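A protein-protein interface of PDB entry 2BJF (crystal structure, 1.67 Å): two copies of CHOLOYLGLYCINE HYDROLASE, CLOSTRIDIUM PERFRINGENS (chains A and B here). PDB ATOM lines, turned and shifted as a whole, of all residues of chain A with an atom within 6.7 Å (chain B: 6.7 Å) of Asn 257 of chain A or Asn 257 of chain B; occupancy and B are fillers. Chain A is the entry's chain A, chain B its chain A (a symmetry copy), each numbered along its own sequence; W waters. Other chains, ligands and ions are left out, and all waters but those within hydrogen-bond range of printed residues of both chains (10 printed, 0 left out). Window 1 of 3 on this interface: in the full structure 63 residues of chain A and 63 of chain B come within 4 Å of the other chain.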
ATOM      1  N   ASN A  19     -14.100  15.433  19.555  1.00  0.00           N
ATOM      2  CA  ASN A  19     -13.064  16.427  19.316  1.00  0.00           C
ATOM      3  C   ASN A  19     -13.730  17.783  19.140  1.00  0.00           C
ATOM      4  O   ASN A  19     -14.721  17.900  18.412  1.00  0.00           O
ATOM      5  CB  ASN A  19     -12.285  16.107  18.036  1.00  0.00           C
ATOM      6  CG  ASN A  19     -11.221  15.042  18.233  1.00  0.00           C
ATOM      7  OD1 ASN A  19     -10.871  14.681  19.356  1.00  0.00           O
ATOM      8  ND2 ASN A  19     -10.693  14.538  17.124  1.00  0.00           N
ATOM      9  N   PHE A 223      -8.276  16.968   6.403  1.00  0.00           N
ATOM     10  CA  PHE A 223      -9.011  17.310   7.618  1.00  0.00           C
ATOM     11  C   PHE A 223     -10.409  17.881   7.365  1.00  0.00           C
ATOM     12  O   PHE A 223     -11.026  18.433   8.281  1.00  0.00           O
ATOM     13  CB  PHE A 223      -8.178  18.260   8.492  1.00  0.00           C
ATOM     14  CG  PHE A 223      -6.854  17.688   8.917  1.00  0.00           C
ATOM     15  CD1 PHE A 223      -6.761  16.886  10.051  1.00  0.00           C
ATOM     16  CD2 PHE A 223      -5.700  17.945   8.180  1.00  0.00           C
ATOM     17  CE1 PHE A 223      -5.538  16.346  10.446  1.00  0.00           C
ATOM     18  CE2 PHE A 223      -4.471  17.410   8.568  1.00  0.00           C
ATOM     19  CZ  PHE A 223      -4.391  16.613   9.704  1.00  0.00           C
ATOM     20  N   ARG A 231     -12.815   8.330   7.931  1.00  0.00           N
ATOM     21  CA  ARG A 231     -11.760   7.753   8.763  1.00  0.00           C
ATOM     22  C   ARG A 231     -12.279   7.232  10.103  1.00  0.00           C
ATOM     23  O   ARG A 231     -12.028   6.081  10.454  1.00  0.00           O
ATOM     24  CB  ARG A 231     -10.602   8.737   8.969  1.00  0.00           C
ATOM     25  CG  ARG A 231      -9.798   9.007   7.702  1.00  0.00           C
ATOM     26  CD  ARG A 231      -8.311   9.237   7.995  1.00  0.00           C
ATOM     27  NE  ARG A 231      -8.057  10.369   8.891  1.00  0.00           N
ATOM     28  CZ  ARG A 231      -8.066  11.650   8.525  1.00  0.00           C
ATOM     29  NH1 ARG A 231      -8.335  12.000   7.271  1.00  0.00           N
ATOM     30  NH2 ARG A 231      -7.810  12.591   9.423  1.00  0.00           N
ATOM     31  N   ILE A 250      -8.868   4.475  26.764  1.00  0.00           N
ATOM     32  CA  ILE A 250      -7.798   5.017  25.926  1.00  0.00           C
ATOM     33  C   ILE A 250      -8.033   4.796  24.424  1.00  0.00           C
ATOM     34  O   ILE A 250      -7.604   5.608  23.604  1.00  0.00           O
ATOM     35  CB  ILE A 250      -6.382   4.524  26.375  1.00  0.00           C
ATOM     36  CG1 ILE A 250      -5.282   5.463  25.861  1.00  0.00           C
ATOM     37  CG2 ILE A 250      -6.123   3.077  25.950  1.00  0.00           C
ATOM     38  CD1 ILE A 250      -5.353   6.883  26.413  1.00  0.00           C
ATOM     39  N   PHE A 252     -10.797   5.085  22.796  1.00  0.00           N
ATOM     40  CA  PHE A 252     -11.616   6.216  22.368  1.00  0.00           C
ATOM     41  C   PHE A 252     -10.727   7.364  21.887  1.00  0.00           C
ATOM     42  O   PHE A 252     -10.963   7.941  20.825  1.00  0.00           O
ATOM     43  CB  PHE A 252     -12.505   6.665  23.533  1.00  0.00           C
ATOM     44  CG  PHE A 252     -13.567   7.660  23.157  1.00  0.00           C
ATOM     45  CD1 PHE A 252     -14.860   7.235  22.870  1.00  0.00           C
ATOM     46  CD2 PHE A 252     -13.287   9.026  23.127  1.00  0.00           C
ATOM     47  CE1 PHE A 252     -15.855   8.150  22.535  1.00  0.00           C
ATOM     48  CE2 PHE A 252     -14.275   9.948  22.791  1.00  0.00           C
ATOM     49  CZ  PHE A 252     -15.560   9.508  22.493  1.00  0.00           C
ATOM     50  N   PHE A 253      -9.694   7.672  22.669  1.00  0.00           N
ATOM     51  CA  PHE A 253      -8.766   8.753  22.345  1.00  0.00           C
ATOM     52  C   PHE A 253      -7.888   8.425  21.139  1.00  0.00           C
ATOM     53  O   PHE A 253      -7.596   9.304  20.328  1.00  0.00           O
ATOM     54  CB  PHE A 253      -7.924   9.123  23.571  1.00  0.00           C
ATOM     55  CG  PHE A 253      -8.694   9.880  24.619  1.00  0.00           C
ATOM     56  CD1 PHE A 253      -8.630  11.270  24.676  1.00  0.00           C
ATOM     57  CD2 PHE A 253      -9.498   9.206  25.537  1.00  0.00           C
ATOM     58  CE1 PHE A 253      -9.351  11.978  25.639  1.00  0.00           C
ATOM     59  CE2 PHE A 253     -10.222   9.905  26.503  1.00  0.00           C
ATOM     60  CZ  PHE A 253     -10.148  11.294  26.552  1.00  0.00           C
ATOM     61  N   HIS A 254      -7.485   7.162  21.012  1.00  0.00           N
ATOM     62  CA  HIS A 254      -6.713   6.724  19.846  1.00  0.00           C
ATOM     63  C   HIS A 254      -7.472   6.932  18.539  1.00  0.00           C
ATOM     64  O   HIS A 254      -6.897   7.388  17.551  1.00  0.00           O
ATOM     65  CB  HIS A 254      -6.269   5.267  19.988  1.00  0.00           C
ATOM     66  CG  HIS A 254      -5.102   5.084  20.907  1.00  0.00           C
ATOM     67  ND1 HIS A 254      -3.827   5.490  20.577  1.00  0.00           N
ATOM     68  CD2 HIS A 254      -5.016   4.537  22.142  1.00  0.00           C
ATOM     69  CE1 HIS A 254      -3.006   5.208  21.573  1.00  0.00           C
ATOM     70  NE2 HIS A 254      -3.702   4.627  22.534  1.00  0.00           N
ATOM     71  N   ILE A 255      -8.765   6.611  18.546  1.00  0.00           N
ATOM     72  CA  ILE A 255      -9.614   6.812  17.370  1.00  0.00           C
ATOM     73  C   ILE A 255      -9.695   8.298  17.004  1.00  0.00           C
ATOM     74  O   ILE A 255      -9.438   8.676  15.859  1.00  0.00           O
ATOM     75  CB  ILE A 255     -11.035   6.211  17.567  1.00  0.00           C
ATOM     76  CG1 ILE A 255     -10.960   4.683  17.673  1.00  0.00           C
ATOM     77  CG2 ILE A 255     -11.952   6.609  16.414  1.00  0.00           C
ATOM     78  CD1 ILE A 255     -12.253   4.018  18.141  1.00  0.00           C
ATOM     79  N   LEU A 256     -10.031   9.136  17.981  1.00  0.00           N
ATOM     80  CA  LEU A 256     -10.190  10.569  17.726  1.00  0.00           C
ATOM     81  C   LEU A 256      -8.884  11.300  17.401  1.00  0.00           C
ATOM     82  O   LEU A 256      -8.900  12.294  16.673  1.00  0.00           O
ATOM     83  CB  LEU A 256     -10.941  11.258  18.871  1.00  0.00           C
ATOM     84  CG  LEU A 256     -12.447  10.973  18.969  1.00  0.00           C
ATOM     85  CD1 LEU A 256     -13.065  11.799  20.078  1.00  0.00           C
ATOM     86  CD2 LEU A 256     -13.172  11.246  17.655  1.00  0.00           C
ATOM     87  N   ASN A 257      -7.762  10.806  17.928  1.00  0.00           N
ATOM     88  CA  ASN A 257      -6.442  11.368  17.607  1.00  0.00           C
ATOM     89  C   ASN A 257      -6.168  11.362  16.100  1.00  0.00           C
ATOM     90  O   ASN A 257      -5.515  12.265  15.575  1.00  0.00           O
ATOM     91  CB  ASN A 257      -5.318  10.608  18.326  1.00  0.00           C
ATOM     92  CG  ASN A 257      -5.194  10.960  19.811  1.00  0.00           C
ATOM     93  OD1 ASN A 257      -4.378  10.366  20.519  1.00  0.00           O
ATOM     94  ND2 ASN A 257      -5.992  11.913  20.285  1.00  0.00           N
ATOM     95  N   ASN A 258      -6.675  10.340  15.413  1.00  0.00           N
ATOM     96  CA  ASN A 258      -6.451  10.182  13.980  1.00  0.00           C
ATOM     97  C   ASN A 258      -7.082  11.294  13.143  1.00  0.00           C
ATOM     98  O   ASN A 258      -6.604  11.603  12.049  1.00  0.00           O
ATOM     99  CB  ASN A 258      -6.956   8.818  13.511  1.00  0.00           C
ATOM    100  CG  ASN A 258      -6.694   8.577  12.038  1.00  0.00           C
ATOM    101  OD1 ASN A 258      -7.580   8.766  11.203  1.00  0.00           O
ATOM    102  ND2 ASN A 258      -5.470   8.182  11.708  1.00  0.00           N
ATOM    103  N   VAL A 259      -8.153  11.890  13.663  1.00  0.00           N
ATOM    104  CA  VAL A 259      -8.857  12.966  12.961  1.00  0.00           C
ATOM    105  C   VAL A 259      -8.671  14.332  13.631  1.00  0.00           C
ATOM    106  O   VAL A 259      -9.351  15.302  13.289  1.00  0.00           O
ATOM    107  CB  VAL A 259     -10.367  12.643  12.761  1.00  0.00           C
ATOM    108  CG1 VAL A 259     -10.545  11.516  11.746  1.00  0.00           C
ATOM    109  CG2 VAL A 259     -11.046  12.297  14.089  1.00  0.00           C
ATOM    110  N   ALA A 260      -7.732  14.400  14.574  1.00  0.00           N
ATOM    111  CA  ALA A 260      -7.422  15.643  15.273  1.00  0.00           C
ATOM    112  C   ALA A 260      -6.629  16.605  14.389  1.00  0.00           C
ATOM    113  O   ALA A 260      -5.737  16.189  13.647  1.00  0.00           O
ATOM    114  CB  ALA A 260      -6.663  15.352  16.565  1.00  0.00           C
ATOM    115  N   MET A 261      -6.970  17.889  14.465  1.00  0.00           N
ATOM    116  CA  MET A 261      -6.257  18.924  13.719  1.00  0.00           C
ATOM    117  C   MET A 261      -4.975  19.335  14.437  1.00  0.00           C
ATOM    118  O   MET A 261      -4.940  19.410  15.670  1.00  0.00           O
ATOM    119  CB  MET A 261      -7.148  20.144  13.484  1.00  0.00           C
ATOM    120  CG  MET A 261      -8.323  19.877  12.563  1.00  0.00           C
ATOM    121  SD  MET A 261      -9.406  21.305  12.412  1.00  0.00           S
ATOM    122  CE  MET A 261     -10.762  20.586  11.494  1.00  0.00           C
ATOM    123  N   VAL A 262      -3.938  19.604  13.648  1.00  0.00           N
ATOM    124  CA  VAL A 262      -2.592  19.900  14.145  1.00  0.00           C
ATOM    125  C   VAL A 262      -2.206  21.331  13.768  1.00  0.00           C
ATOM    126  O   VAL A 262      -2.432  21.758  12.633  1.00  0.00           O
ATOM    127  CB  VAL A 262      -1.553  18.903  13.556  1.00  0.00           C
ATOM    128  CG1 VAL A 262      -0.165  19.142  14.137  1.00  0.00           C
ATOM    129  CG2 VAL A 262      -1.984  17.458  13.799  1.00  0.00           C
ATOM    130  N   THR A 279     -10.441  17.009  23.655  1.00  0.00           N
ATOM    131  CA  THR A 279     -11.102  15.752  23.350  1.00  0.00           C
ATOM    132  C   THR A 279     -11.793  15.276  24.619  1.00  0.00           C
ATOM    133  O   THR A 279     -11.142  15.059  25.643  1.00  0.00           O
ATOM    134  CB  THR A 279     -10.098  14.693  22.857  1.00  0.00           C
ATOM    135  OG1 THR A 279      -9.412  15.187  21.700  1.00  0.00           O
ATOM    136  CG2 THR A 279     -10.807  13.390  22.501  1.00  0.00           C
ATOM    137  N   ASN A 292      -8.991  15.650  27.700  1.00  0.00           N
ATOM    138  CA  ASN A 292      -7.680  16.284  27.651  1.00  0.00           C
ATOM    139  C   ASN A 292      -7.724  17.471  26.689  1.00  0.00           C
ATOM    140  O   ASN A 292      -8.761  17.726  26.071  1.00  0.00           O
ATOM    141  CB  ASN A 292      -6.565  15.280  27.315  1.00  0.00           C
ATOM    142  CG  ASN A 292      -6.680  14.694  25.911  1.00  0.00           C
ATOM    143  OD1 ASN A 292      -7.520  15.100  25.105  1.00  0.00           O
ATOM    144  ND2 ASN A 292      -5.817  13.726  25.616  1.00  0.00           N
ATOM    145  N   ASN A 297      -2.114  16.795  27.335  1.00  0.00           N
ATOM    146  CA  ASN A 297      -2.676  15.531  26.871  1.00  0.00           C
ATOM    147  C   ASN A 297      -3.054  14.531  27.966  1.00  0.00           C
ATOM    148  O   ASN A 297      -3.693  13.517  27.672  1.00  0.00           O
ATOM    149  CB  ASN A 297      -1.769  14.877  25.818  1.00  0.00           C
ATOM    150  CG  ASN A 297      -0.419  14.460  26.375  1.00  0.00           C
ATOM    151  OD1 ASN A 297       0.098  15.061  27.317  1.00  0.00           O
ATOM    152  ND2 ASN A 297       0.167  13.429  25.777  1.00  0.00           N
ATOM    153  N   ASN B  19       7.529   7.335  16.581  1.00  0.00           N
ATOM    154  CA  ASN B  19       6.497   6.343  16.845  1.00  0.00           C
ATOM    155  C   ASN B  19       7.105   4.959  16.673  1.00  0.00           C
ATOM    156  O   ASN B  19       7.810   4.706  15.691  1.00  0.00           O
ATOM    157  CB  ASN B  19       5.338   6.483  15.852  1.00  0.00           C
ATOM    158  CG  ASN B  19       4.368   7.592  16.217  1.00  0.00           C
ATOM    159  OD1 ASN B  19       4.391   8.130  17.324  1.00  0.00           O
ATOM    160  ND2 ASN B  19       3.497   7.934  15.275  1.00  0.00           N
ATOM    161  N   PHE B 223      -2.192   3.954   6.416  1.00  0.00           N
ATOM    162  CA  PHE B 223      -1.094   3.783   7.366  1.00  0.00           C
ATOM    163  C   PHE B 223       0.161   3.145   6.766  1.00  0.00           C
ATOM    164  O   PHE B 223       1.054   2.723   7.506  1.00  0.00           O
ATOM    165  CB  PHE B 223      -1.576   2.999   8.597  1.00  0.00           C
ATOM    166  CG  PHE B 223      -2.706   3.664   9.334  1.00  0.00           C
ATOM    167  CD1 PHE B 223      -2.448   4.632  10.300  1.00  0.00           C
ATOM    168  CD2 PHE B 223      -4.029   3.326   9.058  1.00  0.00           C
ATOM    169  CE1 PHE B 223      -3.491   5.257  10.981  1.00  0.00           C
ATOM    170  CE2 PHE B 223      -5.080   3.946   9.736  1.00  0.00           C
ATOM    171  CZ  PHE B 223      -4.809   4.909  10.700  1.00  0.00           C
ATOM    172  N   ARG B 231       2.376  12.605   5.054  1.00  0.00           N
ATOM    173  CA  ARG B 231       1.631  13.329   6.084  1.00  0.00           C
ATOM    174  C   ARG B 231       2.542  14.036   7.088  1.00  0.00           C
ATOM    175  O   ARG B 231       2.388  15.233   7.321  1.00  0.00           O
ATOM    176  CB  ARG B 231       0.627  12.419   6.801  1.00  0.00           C
ATOM    177  CG  ARG B 231      -0.536  11.979   5.919  1.00  0.00           C
ATOM    178  CD  ARG B 231      -1.842  11.834   6.708  1.00  0.00           C
ATOM    179  NE  ARG B 231      -1.763  10.860   7.800  1.00  0.00           N
ATOM    180  CZ  ARG B 231      -1.841   9.538   7.652  1.00  0.00           C
ATOM    181  NH1 ARG B 231      -1.982   8.994   6.447  1.00  0.00           N
ATOM    182  NH2 ARG B 231      -1.769   8.752   8.718  1.00  0.00           N
ATOM    183  N   ILE B 250       4.629  19.398  23.327  1.00  0.00           N
ATOM    184  CA  ILE B 250       3.359  18.761  22.974  1.00  0.00           C
ATOM    185  C   ILE B 250       3.091  18.743  21.461  1.00  0.00           C
ATOM    186  O   ILE B 250       2.441  17.826  20.959  1.00  0.00           O
ATOM    187  CB  ILE B 250       2.152  19.353  23.775  1.00  0.00           C
ATOM    188  CG1 ILE B 250       0.970  18.374  23.794  1.00  0.00           C
ATOM    189  CG2 ILE B 250       1.733  20.724  23.240  1.00  0.00           C
ATOM    190  CD1 ILE B 250       1.253  17.054  24.504  1.00  0.00           C
ATOM    191  N   PHE B 252       5.187  18.138  19.092  1.00  0.00           N
ATOM    192  CA  PHE B 252       5.853  16.934  18.600  1.00  0.00           C
ATOM    193  C   PHE B 252       4.886  15.749  18.614  1.00  0.00           C
ATOM    194  O   PHE B 252       4.780  15.010  17.635  1.00  0.00           O
ATOM    195  CB  PHE B 252       7.082  16.646  19.470  1.00  0.00           C
ATOM    196  CG  PHE B 252       7.990  15.579  18.928  1.00  0.00           C
ATOM    197  CD1 PHE B 252       9.110  15.922  18.177  1.00  0.00           C
ATOM    198  CD2 PHE B 252       7.751  14.232  19.199  1.00  0.00           C
ATOM    199  CE1 PHE B 252       9.966  14.940  17.682  1.00  0.00           C
ATOM    200  CE2 PHE B 252       8.600  13.244  18.708  1.00  0.00           C
ATOM    201  CZ  PHE B 252       9.707  13.600  17.946  1.00  0.00           C
ATOM    202  N   PHE B 253       4.168  15.591  19.725  1.00  0.00           N
ATOM    203  CA  PHE B 253       3.214  14.498  19.888  1.00  0.00           C
ATOM    204  C   PHE B 253       1.984  14.659  18.995  1.00  0.00           C
ATOM    205  O   PHE B 253       1.469  13.674  18.467  1.00  0.00           O
ATOM    206  CB  PHE B 253       2.823  14.341  21.362  1.00  0.00           C
ATOM    207  CG  PHE B 253       3.909  13.734  22.208  1.00  0.00           C
ATOM    208  CD1 PHE B 253       3.903  12.371  22.495  1.00  0.00           C
ATOM    209  CD2 PHE B 253       4.949  14.519  22.702  1.00  0.00           C
ATOM    210  CE1 PHE B 253       4.914  11.800  23.269  1.00  0.00           C
ATOM    211  CE2 PHE B 253       5.964  13.958  23.477  1.00  0.00           C
ATOM    212  CZ  PHE B 253       5.946  12.595  23.760  1.00  0.00           C
ATOM    213  N   HIS B 254       1.531  15.898  18.814  1.00  0.00           N
ATOM    214  CA  HIS B 254       0.412  16.172  17.908  1.00  0.00           C
ATOM    215  C   HIS B 254       0.713  15.746  16.474  1.00  0.00           C
ATOM    216  O   HIS B 254      -0.139  15.159  15.806  1.00  0.00           O
ATOM    217  CB  HIS B 254       0.001  17.644  17.961  1.00  0.00           C
ATOM    218  CG  HIS B 254      -0.810  17.995  19.168  1.00  0.00           C
ATOM    219  ND1 HIS B 254      -2.113  17.576  19.333  1.00  0.00           N
ATOM    220  CD2 HIS B 254      -0.507  18.727  20.265  1.00  0.00           C
ATOM    221  CE1 HIS B 254      -2.574  18.029  20.486  1.00  0.00           C
ATOM    222  NE2 HIS B 254      -1.622  18.732  21.070  1.00  0.00           N
ATOM    223  N   ILE B 255       1.931  16.031  16.013  1.00  0.00           N
ATOM    224  CA  ILE B 255       2.358  15.632  14.671  1.00  0.00           C
ATOM    225  C   ILE B 255       2.355  14.106  14.530  1.00  0.00           C
ATOM    226  O   ILE B 255       1.751  13.563  13.602  1.00  0.00           O
ATOM    227  CB  ILE B 255       3.750  16.219  14.304  1.00  0.00           C
ATOM    228  CG1 ILE B 255       3.676  17.746  14.193  1.00  0.00           C
ATOM    229  CG2 ILE B 255       4.256  15.626  12.992  1.00  0.00           C
ATOM    230  CD1 ILE B 255       5.033  18.442  14.111  1.00  0.00           C
ATOM    231  N   LEU B 256       3.010  13.418  15.463  1.00  0.00           N
ATOM    232  CA  LEU B 256       3.114  11.960  15.393  1.00  0.00           C
ATOM    233  C   LEU B 256       1.793  11.221  15.623  1.00  0.00           C
ATOM    234  O   LEU B 256       1.598  10.128  15.091  1.00  0.00           O
ATOM    235  CB  LEU B 256       4.213  11.435  16.325  1.00  0.00           C
ATOM    236  CG  LEU B 256       5.662  11.693  15.886  1.00  0.00           C
ATOM    237  CD1 LEU B 256       6.627  11.031  16.848  1.00  0.00           C
ATOM    238  CD2 LEU B 256       5.931  11.204  14.466  1.00  0.00           C
ATOM    239  N   ASN B 257       0.889  11.819  16.402  1.00  0.00           N
ATOM    240  CA  ASN B 257      -0.449  11.248  16.615  1.00  0.00           C
ATOM    241  C   ASN B 257      -1.196  11.030  15.296  1.00  0.00           C
ATOM    242  O   ASN B 257      -1.960  10.075  15.154  1.00  0.00           O
ATOM    243  CB  ASN B 257      -1.299  12.137  17.533  1.00  0.00           C
ATOM    244  CG  ASN B 257      -0.928  12.021  19.014  1.00  0.00           C
ATOM    245  OD1 ASN B 257      -1.486  12.737  19.848  1.00  0.00           O
ATOM    246  ND2 ASN B 257       0.005  11.131  19.345  1.00  0.00           N
ATOM    247  N   ASN B 258      -0.964  11.922  14.333  1.00  0.00           N
ATOM    248  CA  ASN B 258      -1.643  11.864  13.044  1.00  0.00           C
ATOM    249  C   ASN B 258      -1.288  10.621  12.228  1.00  0.00           C
ATOM    250  O   ASN B 258      -2.085  10.161  11.408  1.00  0.00           O
ATOM    251  CB  ASN B 258      -1.352  13.127  12.233  1.00  0.00           C
ATOM    252  CG  ASN B 258      -2.082  13.146  10.906  1.00  0.00           C
ATOM    253  OD1 ASN B 258      -1.509  12.810   9.868  1.00  0.00           O
ATOM    254  ND2 ASN B 258      -3.356  13.518  10.932  1.00  0.00           N
ATOM    255  N   VAL B 259      -0.092  10.085  12.459  1.00  0.00           N
ATOM    256  CA  VAL B 259       0.375   8.897  11.741  1.00  0.00           C
ATOM    257  C   VAL B 259       0.450   7.654  12.636  1.00  0.00           C
ATOM    258  O   VAL B 259       1.008   6.626  12.245  1.00  0.00           O
ATOM    259  CB  VAL B 259       1.730   9.146  11.016  1.00  0.00           C
ATOM    260  CG1 VAL B 259       1.542  10.100   9.838  1.00  0.00           C
ATOM    261  CG2 VAL B 259       2.793   9.674  11.984  1.00  0.00           C
ATOM    262  N   ALA B 260      -0.132   7.755  13.829  1.00  0.00           N
ATOM    263  CA  ALA B 260      -0.167   6.642  14.773  1.00  0.00           C
ATOM    264  C   ALA B 260      -1.178   5.578  14.351  1.00  0.00           C
ATOM    265  O   ALA B 260      -2.273   5.898  13.883  1.00  0.00           O
ATOM    266  CB  ALA B 260      -0.475   7.147  16.180  1.00  0.00           C
ATOM    267  N   MET B 261      -0.798   4.312  14.508  1.00  0.00           N
ATOM    268  CA  MET B 261      -1.688   3.193  14.200  1.00  0.00           C
ATOM    269  C   MET B 261      -2.657   2.930  15.348  1.00  0.00           C
ATOM    270  O   MET B 261      -2.290   3.046  16.523  1.00  0.00           O
ATOM    271  CB  MET B 261      -0.889   1.930  13.880  1.00  0.00           C
ATOM    272  CG  MET B 261      -0.082   2.022  12.599  1.00  0.00           C
ATOM    273  SD  MET B 261       0.930   0.561  12.327  1.00  0.00           S
ATOM    274  CE  MET B 261       1.898   1.095  10.921  1.00  0.00           C
ATOM    275  N   VAL B 262      -3.886   2.569  14.987  1.00  0.00           N
ATOM    276  CA  VAL B 262      -4.992   2.388  15.932  1.00  0.00           C
ATOM    277  C   VAL B 262      -5.442   0.927  15.924  1.00  0.00           C
ATOM    278  O   VAL B 262      -5.584   0.325  14.856  1.00  0.00           O
ATOM    279  CB  VAL B 262      -6.191   3.309  15.565  1.00  0.00           C
ATOM    280  CG1 VAL B 262      -7.309   3.197  16.593  1.00  0.00           C
ATOM    281  CG2 VAL B 262      -5.740   4.763  15.432  1.00  0.00           C
ATOM    282  N   THR B 279       5.432   6.499  21.834  1.00  0.00           N
ATOM    283  CA  THR B 279       5.928   7.677  21.144  1.00  0.00           C
ATOM    284  C   THR B 279       6.980   8.324  22.032  1.00  0.00           C
ATOM    285  O   THR B 279       6.689   8.712  23.166  1.00  0.00           O
ATOM    286  CB  THR B 279       4.791   8.674  20.845  1.00  0.00           C
ATOM    287  OG1 THR B 279       3.781   8.026  20.062  1.00  0.00           O
ATOM    288  CG2 THR B 279       5.313   9.888  20.084  1.00  0.00           C
ATOM    289  N   ASN B 292       5.334   8.498  25.872  1.00  0.00           N
ATOM    290  CA  ASN B 292       4.093   7.897  26.348  1.00  0.00           C
ATOM    291  C   ASN B 292       3.855   6.577  25.617  1.00  0.00           C
ATOM    292  O   ASN B 292       4.643   6.204  24.743  1.00  0.00           O
ATOM    293  CB  ASN B 292       2.905   8.866  26.240  1.00  0.00           C
ATOM    294  CG  ASN B 292       2.546   9.228  24.802  1.00  0.00           C
ATOM    295  OD1 ASN B 292       3.089   8.682  23.840  1.00  0.00           O
ATOM    296  ND2 ASN B 292       1.608  10.161  24.657  1.00  0.00           N
ATOM    297  N   ASN B 297      -1.260   7.487  27.929  1.00  0.00           N
ATOM    298  CA  ASN B 297      -0.911   8.650  27.120  1.00  0.00           C
ATOM    299  C   ASN B 297      -0.225   9.796  27.868  1.00  0.00           C
ATOM    300  O   ASN B 297       0.258  10.737  27.232  1.00  0.00           O
ATOM    301  CB  ASN B 297      -2.126   9.158  26.330  1.00  0.00           C
ATOM    302  CG  ASN B 297      -3.234   9.690  27.223  1.00  0.00           C
ATOM    303  OD1 ASN B 297      -3.404   9.254  28.362  1.00  0.00           O
ATOM    304  ND2 ASN B 297      -4.008  10.631  26.696  1.00  0.00           N
HETATM  305  O   HOH W   1      -0.978  12.762  23.084  1.00  0.00           O
HETATM  306  O   HOH W   2      -3.090   5.405  17.881  1.00  0.00           O
HETATM  307  O   HOH W   3      -5.020  13.497   8.725  1.00  0.00           O
HETATM  308  O   HOH W   4      -4.599  10.762  10.208  1.00  0.00           O
HETATM  309  O   HOH W   5      -3.684  17.267  17.041  1.00  0.00           O
HETATM  310  O   HOH W   6      -4.265  13.960  13.771  1.00  0.00           O
HETATM  311  O   HOH W   7      -3.682   8.156  14.133  1.00  0.00           O
HETATM  312  O   HOH W   8      -5.015  10.563   7.725  1.00  0.00           O
HETATM  313  O   HOH W   9      -3.813  10.849  23.709  1.00  0.00           O
HETATM  314  O   HOH W  10      -4.610   7.821   9.106  1.00  0.00           O
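Of the printed residues of chain B, Asn 257 of chain A touches Asn 257. Asn 257 of chain B touches one residue of chain A. Of the printed residues of chain B, Asn 292 of chain A touches Asn 297 (3.7 Å). Of the printed residues of chain A, Asn 258 of chain B touches Phe 223 and Asn 258. The nearest printed residue of chain A that does not touch His 254 of chain B is Met 261 of chain A (5.0 Å).
Ile 250 of chain A touches Asn 297 of chain B, and with the chains exchanged Asn 297 of chain A touches Ile 250 of chain B. His 254 of chain A touches Val 262 of chain B, and with the chains exchanged Val 262 of chain A touches His 254 of chain B. Asn 257 of chain B touches its own counterpart, Asn 257 of chain A. Positions printed for both chains: 19, 223, 231, 250, 252, 253, 254, 255, 256, 257, 258, 259, 260, 261, 262, 279, 292 and 297.
ND2 of Asn 258 of chain B touches CZ of Phe 223 of chain A (3.5 Å). O of His 254 of chain A touches CG2 of Val 262 of chain B, 3.6 Å away. O of Asn 258 of chain A touches ND2 of Asn 258 of chain B, at 3.9 Å. CG2 of Val 262 of chain A touches O of His 254 of chain B, 3.6 Å away. ND2 of Asn 292 of chain A touches ND2 of Asn 297 of chain B, 3.7 Å away. CG of Asn 297 of chain A touches CD1 of Ile 250 of chain B, at 3.6 Å. Asn 292 of chain B touches Asn 297 of chain A (ND2 to ND2, 3.7 Å).
The guanidinium group of Arg 231 of chain A sits at hydrogen-bond distance from the side-chain amide oxygen of Asn 258 of chain A (2.9 Å). ND2 of Asn 292 of chain A lies within hydrogen-bond range of O of Asn 297 of chain A (3.0 Å). The backbone NH (N) of Thr 279 of chain B sits at hydrogen-bond distance from the backbone carbonyl oxygen (O) of Asn 292 of chain B (3.0 Å).
Of the 18 printed residues of chain B, 8 touch a printed residue of chain A. Of the 18 printed residues of chain A, 8 touch a printed residue of chain B. Among the printed residues, no Asp or Glu carboxylate lies within 4 Å of a Lys or Arg side-chain nitrogen of the other chain.
Water W7 lies within hydrogen-bond range of O of Ala 260 of chain B (2.7 Å), O of Asn 257 of chain B (2.8 Å) and ND2 of Asn 258 of chain A (3.0 Å). Water W5 lies within hydrogen-bond range of ND1 of His 254 of chain B and O of Met 261 of chain A. Water W2 lies within hydrogen-bond range of a ring nitrogen (ND1) of His 254 of chain A (2.8 Å) and the backbone carbonyl oxygen (O) of Met 261 of chain B (2.8 Å). Water W9 bridges ND2 of Asn 297 of chain B (3.0 Å) and OD1 of Asn 257 of chain A (3.3 Å).
ND2 of Asn 297 of chain A is in hydrogen-bond range of O of Asn 297 of chain B (3.1 Å).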
